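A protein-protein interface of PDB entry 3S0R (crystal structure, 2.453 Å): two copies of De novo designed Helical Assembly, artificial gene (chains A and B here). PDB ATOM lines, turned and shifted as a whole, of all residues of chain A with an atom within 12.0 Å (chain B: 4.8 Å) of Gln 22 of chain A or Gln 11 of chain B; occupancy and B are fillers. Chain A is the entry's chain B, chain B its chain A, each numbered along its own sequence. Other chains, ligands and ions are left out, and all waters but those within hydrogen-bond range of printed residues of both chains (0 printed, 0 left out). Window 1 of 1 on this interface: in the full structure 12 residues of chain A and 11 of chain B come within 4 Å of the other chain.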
ATOM      1  N   GLN A  11      20.949   3.570  17.667  1.00  0.00           N
ATOM      2  CA  GLN A  11      20.475   4.889  18.078  1.00  0.00           C
ATOM      3  C   GLN A  11      21.488   5.642  18.925  1.00  0.00           C
ATOM      4  O   GLN A  11      21.997   6.695  18.530  1.00  0.00           O
ATOM      5  CB  GLN A  11      19.188   4.746  18.884  1.00  0.00           C
ATOM      6  CG  GLN A  11      17.971   4.545  18.041  1.00  0.00           C
ATOM      7  CD  GLN A  11      16.900   3.756  18.749  1.00  0.00           C
ATOM      8  OE1 GLN A  11      17.180   3.022  19.697  1.00  0.00           O
ATOM      9  NE2 GLN A  11      15.665   3.893  18.283  1.00  0.00           N
ATOM     10  N   ALA A  13      24.556   5.258  19.658  1.00  0.00           N
ATOM     11  CA  ALA A  13      25.819   5.529  18.982  1.00  0.00           C
ATOM     12  C   ALA A  13      25.619   6.605  17.929  1.00  0.00           C
ATOM     13  O   ALA A  13      26.461   7.486  17.734  1.00  0.00           O
ATOM     14  CB  ALA A  13      26.345   4.264  18.337  1.00  0.00           C
ATOM     15  N   LEU A  14      24.496   6.516  17.239  1.00  0.00           N
ATOM     16  CA  LEU A  14      24.182   7.459  16.183  1.00  0.00           C
ATOM     17  C   LEU A  14      24.150   8.895  16.712  1.00  0.00           C
ATOM     18  O   LEU A  14      24.528   9.841  16.015  1.00  0.00           O
ATOM     19  CB  LEU A  14      22.835   7.102  15.569  1.00  0.00           C
ATOM     20  CG  LEU A  14      22.744   7.316  14.065  1.00  0.00           C
ATOM     21  CD1 LEU A  14      23.760   6.427  13.383  1.00  0.00           C
ATOM     22  CD2 LEU A  14      21.338   7.026  13.561  1.00  0.00           C
ATOM     23  N   GLU A  15      23.693   9.053  17.952  1.00  0.00           N
ATOM     24  CA  GLU A  15      23.572  10.380  18.546  1.00  0.00           C
ATOM     25  C   GLU A  15      24.895  10.873  19.114  1.00  0.00           C
ATOM     26  O   GLU A  15      25.152  12.072  19.170  1.00  0.00           O
ATOM     27  CB  GLU A  15      22.487  10.395  19.625  1.00  0.00           C
ATOM     28  CG  GLU A  15      22.307  11.745  20.331  1.00  0.00           C
ATOM     29  CD  GLU A  15      22.049  12.905  19.367  1.00  0.00           C
ATOM     30  OE1 GLU A  15      22.833  13.877  19.386  1.00  0.00           O
ATOM     31  OE2 GLU A  15      21.064  12.853  18.595  1.00  0.00           O
ATOM     32  N   LYS A  16      25.742   9.961  19.551  1.00  0.00           N
ATOM     33  CA  LYS A  16      27.052  10.396  19.964  1.00  0.00           C
ATOM     34  C   LYS A  16      27.726  10.928  18.712  1.00  0.00           C
ATOM     35  O   LYS A  16      28.487  11.898  18.758  1.00  0.00           O
ATOM     36  CB  LYS A  16      27.844   9.246  20.573  1.00  0.00           C
ATOM     37  CG  LYS A  16      27.415   8.887  21.986  1.00  0.00           C
ATOM     38  CD  LYS A  16      28.176   7.670  22.507  1.00  0.00           C
ATOM     39  CE  LYS A  16      27.641   7.239  23.863  1.00  0.00           C
ATOM     40  NZ  LYS A  16      27.715   5.767  24.061  1.00  0.00           N
ATOM     41  N   ALA A  17      27.404  10.296  17.583  1.00  0.00           N
ATOM     42  CA  ALA A  17      27.957  10.671  16.288  1.00  0.00           C
ATOM     43  C   ALA A  17      27.550  12.074  15.910  1.00  0.00           C
ATOM     44  O   ALA A  17      28.408  12.906  15.632  1.00  0.00           O
ATOM     45  CB  ALA A  17      27.518   9.695  15.216  1.00  0.00           C
ATOM     46  N   GLN A  18      26.247  12.341  15.888  1.00  0.00           N
ATOM     47  CA  GLN A  18      25.769  13.684  15.584  1.00  0.00           C
ATOM     48  C   GLN A  18      26.335  14.680  16.583  1.00  0.00           C
ATOM     49  O   GLN A  18      26.556  15.841  16.247  1.00  0.00           O
ATOM     50  CB  GLN A  18      24.250  13.737  15.578  1.00  0.00           C
ATOM     51  CG  GLN A  18      23.613  13.309  14.268  1.00  0.00           C
ATOM     52  CD  GLN A  18      23.502  14.437  13.247  1.00  0.00           C
ATOM     53  OE1 GLN A  18      24.339  15.341  13.196  1.00  0.00           O
ATOM     54  NE2 GLN A  18      22.464  14.384  12.427  1.00  0.00           N
ATOM     55  N   LEU A  19      26.590  14.219  17.804  1.00  0.00           N
ATOM     56  CA  LEU A  19      27.193  15.074  18.827  1.00  0.00           C
ATOM     57  C   LEU A  19      28.652  15.438  18.526  1.00  0.00           C
ATOM     58  O   LEU A  19      29.041  16.590  18.666  1.00  0.00           O
ATOM     59  CB  LEU A  19      27.064  14.453  20.222  1.00  0.00           C
ATOM     60  CG  LEU A  19      25.730  14.662  20.949  1.00  0.00           C
ATOM     61  CD1 LEU A  19      25.775  14.020  22.316  1.00  0.00           C
ATOM     62  CD2 LEU A  19      25.380  16.135  21.070  1.00  0.00           C
ATOM     63  N   ALA A  20      29.456  14.456  18.124  1.00  0.00           N
ATOM     64  CA  ALA A  20      30.845  14.701  17.750  1.00  0.00           C
ATOM     65  C   ALA A  20      30.863  15.540  16.488  1.00  0.00           C
ATOM     66  O   ALA A  20      31.790  16.317  16.234  1.00  0.00           O
ATOM     67  CB  ALA A  20      31.551  13.399  17.493  1.00  0.00           C
ATOM     68  N   LEU A  21      29.816  15.349  15.701  1.00  0.00           N
ATOM     69  CA  LEU A  21      29.617  16.050  14.449  1.00  0.00           C
ATOM     70  C   LEU A  21      29.526  17.566  14.614  1.00  0.00           C
ATOM     71  O   LEU A  21      30.289  18.327  14.014  1.00  0.00           O
ATOM     72  CB  LEU A  21      28.330  15.557  13.818  1.00  0.00           C
ATOM     73  CG  LEU A  21      28.385  15.769  12.317  1.00  0.00           C
ATOM     74  CD1 LEU A  21      29.816  15.529  11.876  1.00  0.00           C
ATOM     75  CD2 LEU A  21      27.415  14.849  11.594  1.00  0.00           C
ATOM     76  N   GLN A  22      28.562  18.004  15.411  1.00  0.00           N
ATOM     77  CA  GLN A  22      28.422  19.413  15.713  1.00  0.00           C
ATOM     78  C   GLN A  22      29.719  19.962  16.288  1.00  0.00           C
ATOM     79  O   GLN A  22      30.157  21.041  15.906  1.00  0.00           O
ATOM     80  CB  GLN A  22      27.285  19.609  16.706  1.00  0.00           C
ATOM     81  CG  GLN A  22      26.964  21.059  17.017  1.00  0.00           C
ATOM     82  CD  GLN A  22      25.815  21.185  18.009  1.00  0.00           C
ATOM     83  OE1 GLN A  22      25.652  20.336  18.890  1.00  0.00           O
ATOM     84  NE2 GLN A  22      25.013  22.242  17.869  1.00  0.00           N
ATOM     85  N   ALA A  23      30.331  19.205  17.197  1.00  0.00           N
ATOM     86  CA  ALA A  23      31.567  19.617  17.865  1.00  0.00           C
ATOM     87  C   ALA A  23      32.643  20.032  16.872  1.00  0.00           C
ATOM     88  O   ALA A  23      33.262  21.089  17.021  1.00  0.00           O
ATOM     89  CB  ALA A  23      32.084  18.515  18.764  1.00  0.00           C
ATOM     90  N   ALA A  24      32.877  19.191  15.867  1.00  0.00           N
ATOM     91  CA  ALA A  24      33.845  19.510  14.823  1.00  0.00           C
ATOM     92  C   ALA A  24      33.382  20.730  14.033  1.00  0.00           C
ATOM     93  O   ALA A  24      34.153  21.665  13.794  1.00  0.00           O
ATOM     94  CB  ALA A  24      34.038  18.339  13.910  1.00  0.00           C
ATOM     95  N   ARG A  25      32.113  20.713  13.642  1.00  0.00           N
ATOM     96  CA  ARG A  25      31.526  21.828  12.936  1.00  0.00           C
ATOM     97  C   ARG A  25      31.920  23.108  13.637  1.00  0.00           C
ATOM     98  O   ARG A  25      32.634  23.935  13.084  1.00  0.00           O
ATOM     99  CB  ARG A  25      30.006  21.699  12.910  1.00  0.00           C
ATOM    100  CG  ARG A  25      29.490  20.389  12.335  1.00  0.00           C
ATOM    101  CD  ARG A  25      29.548  20.342  10.814  1.00  0.00           C
ATOM    102  NE  ARG A  25      28.707  21.347  10.161  1.00  0.00           N
ATOM    103  CZ  ARG A  25      29.176  22.393   9.477  1.00  0.00           C
ATOM    104  NH1 ARG A  25      30.488  22.583   9.352  1.00  0.00           N
ATOM    105  NH2 ARG A  25      28.336  23.257   8.919  1.00  0.00           N
ATOM    106  N   GLN A  26      31.464  23.259  14.873  1.00  0.00           N
ATOM    107  CA  GLN A  26      31.720  24.470  15.645  1.00  0.00           C
ATOM    108  C   GLN A  26      33.210  24.831  15.738  1.00  0.00           C
ATOM    109  O   GLN A  26      33.588  25.996  15.587  1.00  0.00           O
ATOM    110  CB  GLN A  26      31.106  24.351  17.041  1.00  0.00           C
ATOM    111  CG  GLN A  26      29.592  24.537  17.074  1.00  0.00           C
ATOM    112  CD  GLN A  26      29.140  25.982  16.799  1.00  0.00           C
ATOM    113  OE1 GLN A  26      28.530  26.269  15.766  1.00  0.00           O
ATOM    114  NE2 GLN A  26      29.433  26.887  17.730  1.00  0.00           N
ATOM    115  N   ALA A  27      34.051  23.834  15.991  1.00  0.00           N
ATOM    116  CA  ALA A  27      35.472  24.084  16.129  1.00  0.00           C
ATOM    117  C   ALA A  27      35.895  24.789  14.867  1.00  0.00           C
ATOM    118  O   ALA A  27      36.742  25.683  14.882  1.00  0.00           O
ATOM    119  CB  ALA A  27      36.227  22.777  16.299  1.00  0.00           C
ATOM    120  N   LEU A  28      35.258  24.386  13.776  1.00  0.00           N
ATOM    121  CA  LEU A  28      35.562  24.902  12.452  1.00  0.00           C
ATOM    122  C   LEU A  28      34.963  26.265  12.196  1.00  0.00           C
ATOM    123  O   LEU A  28      35.422  26.997  11.316  1.00  0.00           O
ATOM    124  CB  LEU A  28      35.048  23.946  11.393  1.00  0.00           C
ATOM    125  CG  LEU A  28      36.031  22.830  11.136  1.00  0.00           C
ATOM    126  CD1 LEU A  28      35.918  22.435   9.682  1.00  0.00           C
ATOM    127  CD2 LEU A  28      37.411  23.361  11.455  1.00  0.00           C
ATOM    128  N   LYS A  29      33.910  26.591  12.933  1.00  0.00           N
ATOM    129  CA  LYS A  29      33.377  27.940  12.894  1.00  0.00           C
ATOM    130  C   LYS A  29      34.132  28.803  13.907  1.00  0.00           C
ATOM    131  O   LYS A  29      33.644  29.845  14.335  1.00  0.00           O
ATOM    132  CB  LYS A  29      31.869  27.941  13.154  1.00  0.00           C
ATOM    133  CG  LYS A  29      31.072  27.122  12.133  1.00  0.00           C
ATOM    134  CD  LYS A  29      29.724  27.766  11.803  1.00  0.00           C
ATOM    135  CE  LYS A  29      28.888  26.910  10.844  1.00  0.00           C
ATOM    136  NZ  LYS A  29      28.351  25.671  11.466  1.00  0.00           N
ATOM    137  N   ALA A  30      35.336  28.352  14.274  1.00  0.00           N
ATOM    138  CA  ALA A  30      36.212  29.069  15.199  1.00  0.00           C
ATOM    139  C   ALA A  30      37.658  29.052  14.706  1.00  0.00           C
ATOM    140  O   ALA A  30      38.063  28.146  13.979  1.00  0.00           O
ATOM    141  CB  ALA A  30      36.120  28.464  16.592  1.00  0.00           C
ATOM    142  N   LEU B   7      30.853  18.405   5.925  1.00  0.00           N
ATOM    143  CA  LEU B   7      30.304  18.327   7.266  1.00  0.00           C
ATOM    144  C   LEU B   7      28.795  18.441   7.264  1.00  0.00           C
ATOM    145  O   LEU B   7      28.112  17.538   7.741  1.00  0.00           O
ATOM    146  CB  LEU B   7      30.880  19.442   8.125  1.00  0.00           C
ATOM    147  CG  LEU B   7      32.226  19.153   8.767  1.00  0.00           C
ATOM    148  CD1 LEU B   7      32.732  20.360   9.542  1.00  0.00           C
ATOM    149  CD2 LEU B   7      32.060  17.950   9.667  1.00  0.00           C
ATOM    150  N   GLU B   8      28.286  19.560   6.745  1.00  0.00           N
ATOM    151  CA  GLU B   8      26.854  19.820   6.726  1.00  0.00           C
ATOM    152  C   GLU B   8      26.111  18.610   6.188  1.00  0.00           C
ATOM    153  O   GLU B   8      25.266  18.028   6.871  1.00  0.00           O
ATOM    154  CB  GLU B   8      26.526  21.053   5.882  1.00  0.00           C
ATOM    155  CG  GLU B   8      26.553  22.367   6.654  1.00  0.00           C
ATOM    156  CD  GLU B   8      25.697  23.457   6.006  1.00  0.00           C
ATOM    157  OE1 GLU B   8      25.000  23.166   5.008  1.00  0.00           O
ATOM    158  OE2 GLU B   8      25.721  24.606   6.499  1.00  0.00           O
ATOM    159  N   TYR B   9      26.448  18.234   4.958  1.00  0.00           N
ATOM    160  CA  TYR B   9      25.856  17.067   4.312  1.00  0.00           C
ATOM    161  C   TYR B   9      25.832  15.841   5.222  1.00  0.00           C
ATOM    162  O   TYR B   9      24.816  15.158   5.329  1.00  0.00           O
ATOM    163  CB  TYR B   9      26.606  16.721   3.021  1.00  0.00           C
ATOM    164  CG  TYR B   9      26.058  15.481   2.370  1.00  0.00           C
ATOM    165  CD1 TYR B   9      25.024  15.562   1.455  1.00  0.00           C
ATOM    166  CD2 TYR B   9      26.545  14.228   2.703  1.00  0.00           C
ATOM    167  CE1 TYR B   9      24.499  14.429   0.872  1.00  0.00           C
ATOM    168  CE2 TYR B   9      26.031  13.086   2.119  1.00  0.00           C
ATOM    169  CZ  TYR B   9      25.005  13.193   1.203  1.00  0.00           C
ATOM    170  OH  TYR B   9      24.481  12.067   0.612  1.00  0.00           O
ATOM    171  N   ALA B  10      26.959  15.557   5.862  1.00  0.00           N
ATOM    172  CA  ALA B  10      27.029  14.435   6.774  1.00  0.00           C
ATOM    173  C   ALA B  10      25.903  14.494   7.796  1.00  0.00           C
ATOM    174  O   ALA B  10      25.103  13.573   7.901  1.00  0.00           O
ATOM    175  CB  ALA B  10      28.369  14.399   7.462  1.00  0.00           C
ATOM    176  N   GLN B  11      25.833  15.587   8.538  1.00  0.00           N
ATOM    177  CA  GLN B  11      24.831  15.715   9.581  1.00  0.00           C
ATOM    178  C   GLN B  11      23.444  15.369   9.068  1.00  0.00           C
ATOM    179  O   GLN B  11      22.684  14.672   9.732  1.00  0.00           O
ATOM    180  CB  GLN B  11      24.850  17.126  10.156  1.00  0.00           C
ATOM    181  CG  GLN B  11      26.253  17.643  10.405  1.00  0.00           C
ATOM    182  CD  GLN B  11      26.347  18.516  11.631  1.00  0.00           C
ATOM    183  OE1 GLN B  11      26.923  19.602  11.590  1.00  0.00           O
ATOM    184  NE2 GLN B  11      25.776  18.048  12.731  1.00  0.00           N
ATOM    185  N   GLN B  12      23.130  15.853   7.874  1.00  0.00           N
ATOM    186  CA  GLN B  12      21.811  15.652   7.285  1.00  0.00           C
ATOM    187  C   GLN B  12      21.566  14.173   7.003  1.00  0.00           C
ATOM    188  O   GLN B  12      20.508  13.622   7.325  1.00  0.00           O
ATOM    189  CB  GLN B  12      21.693  16.454   5.988  1.00  0.00           C
ATOM    190  CG  GLN B  12      22.208  17.881   6.104  1.00  0.00           C
ATOM    191  CD  GLN B  12      22.407  18.532   4.752  1.00  0.00           C
ATOM    192  OE1 GLN B  12      21.972  18.009   3.725  1.00  0.00           O
ATOM    193  NE2 GLN B  12      23.071  19.681   4.743  1.00  0.00           N
ATOM    194  N   ALA B  13      22.556  13.540   6.385  1.00  0.00           N
ATOM    195  CA  ALA B  13      22.496  12.118   6.123  1.00  0.00           C
ATOM    196  C   ALA B  13      22.164  11.453   7.439  1.00  0.00           C
ATOM    197  O   ALA B  13      21.179  10.731   7.563  1.00  0.00           O
ATOM    198  CB  ALA B  13      23.830  11.625   5.602  1.00  0.00           C
ATOM    199  N   LEU B  14      22.995  11.723   8.435  1.00  0.00           N
ATOM    200  CA  LEU B  14      22.758  11.207   9.763  1.00  0.00           C
ATOM    201  C   LEU B  14      21.316  11.441  10.142  1.00  0.00           C
ATOM    202  O   LEU B  14      20.643  10.543  10.644  1.00  0.00           O
ATOM    203  CB  LEU B  14      23.667  11.892  10.765  1.00  0.00           C
ATOM    204  CG  LEU B  14      24.855  11.041  11.193  1.00  0.00           C
ATOM    205  CD1 LEU B  14      25.885  11.883  11.930  1.00  0.00           C
ATOM    206  CD2 LEU B  14      24.344   9.918  12.066  1.00  0.00           C
ATOM    207  N   GLU B  15      20.825  12.642   9.879  1.00  0.00           N
ATOM    208  CA  GLU B  15      19.463  12.947  10.266  1.00  0.00           C
ATOM    209  C   GLU B  15      18.473  11.917   9.759  1.00  0.00           C
ATOM    210  O   GLU B  15      17.659  11.406  10.510  1.00  0.00           O
ATOM    211  CB  GLU B  15      19.060  14.349   9.831  1.00  0.00           C
ATOM    212  CG  GLU B  15      19.220  15.351  10.940  1.00  0.00           C
ATOM    213  CD  GLU B  15      18.758  14.794  12.275  1.00  0.00           C
ATOM    214  OE1 GLU B  15      17.775  14.017  12.299  1.00  0.00           O
ATOM    215  OE2 GLU B  15      19.381  15.124  13.304  1.00  0.00           O
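The backbone carbonyl oxygen (O) of Gln 11 of chain B sits at hydrogen-bond distance from the side-chain amide nitrogen (NE2) of Gln 18 of chain A (2.7 Å).
OE2 of Glu 8 of chain B lies within salt-bridge range of NH2 of Arg 25 of chain A, 3.8 Å away.
OE2 of Glu 15 of chain B is in hydrogen-bond range of NE2 of Gln 18 of chain A.
The side-chain amide oxygen (OE1) of Gln 11 of chain B lies close to the guanidinium group (NE) of Arg 25 of chain A (2.9 Å).
The side-chain amide nitrogen of Gln 12 of chain B lies close to the backbone carbonyl oxygen of Glu 8 of chain B.
Leu 14 of chain A touches Leu 14 of chain B (CG to CD2, 3.7 Å).
Gln 18 of chain A touches Leu 14 of chain B.
CD2 of Leu 7 of chain B touches CD1 of Leu 21 of chain A (3.97 Å).
CD2 of Leu 21 of chain A touches CG of Gln 11 of chain B (3.3 Å).
Leu 21 of chain A touches Leu 14 of chain B (CD2 to CD1, 3.4 Å).
Gln 22 of chain A touches Gln 11 of chain B (N to NE2, 3.9 Å).
Leu 7 of chain B touches Arg 25 of chain A (CB to CD, 3.1 Å).
CD1 of Leu 28 of chain A touches CD1 of Leu 7 of chain B, at 3.8 Å.
Gln 22 of chain A touches one residue of chain B.
Gln 11 of chain B touches four residues of chain A.
Leu 7 of chain B touches just these residues of chain A: Leu 21, Arg 25 and Leu 28.
Of chain A, only Arg 25 comes within 4 Å of Glu 8 of chain B.
No residue of chain A comes within 4 Å of Ala 10 of chain B.
No residue of chain A comes within 4 Å of Gln 12 of chain B.
Leu 14 of chain B touches just these residues of chain A: Leu 14 (3.7 Å), Gln 18 (3.2 Å) and Leu 21 (3.4 Å).
Printed residues of chain B within 4 Å of Leu 14 of chain A: Leu 14 (3.7 Å).
Of the printed residues of chain B, Leu 28 of chain A touches Leu 7.
Of the printed residues of chain B, Arg 25 of chain A touches Leu 7 (3.1 Å), Glu 8 (3.0 Å) and Gln 11 (2.8 Å).
Printed residues of chain B within 4 Å of Gln 18 of chain A: Gln 11 (2.7 Å), Leu 14 (3.2 Å) and Glu 15 (3.3 Å).
Of the printed residues of chain B, Leu 21 of chain A touches Leu 7 (3.97 Å), Gln 11 (3.3 Å) and Leu 14 (3.4 Å).
Gln 26 of chain A touches none of the printed residues of chain B.
The nearest printed residue of chain B that does not touch Gln 22 of chain A is Leu 7 of chain B (6.7 Å).
Of the 19 printed residues of chain A, 6 touch a printed residue of chain B.
Of the 9 printed residues of chain B, 5 touch a printed residue of chain A.
Printed residues of chain B that touch a printed residue of chain A: Leu 7, Glu 8, Gln 11, Leu 14 and Glu 15.
Hydrophobic or aromatic side chains of chain B that line the printed part of chain A: Leu 7 and Leu 14.
Among the printed residues, Asp or Glu carboxylates within 4 Å of a Lys or Arg side-chain nitrogen of the other chain: Arg 25 of chain A with Glu 8 of chain B (3.8 Å).
Leu 14 of chain B touches its own counterpart, Leu 14 of chain A.
4 positions are printed for both chains.
Of the 12 pairs that touch across the chains among the printed residues, 1 has its exchanged pair printed and touching as well.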
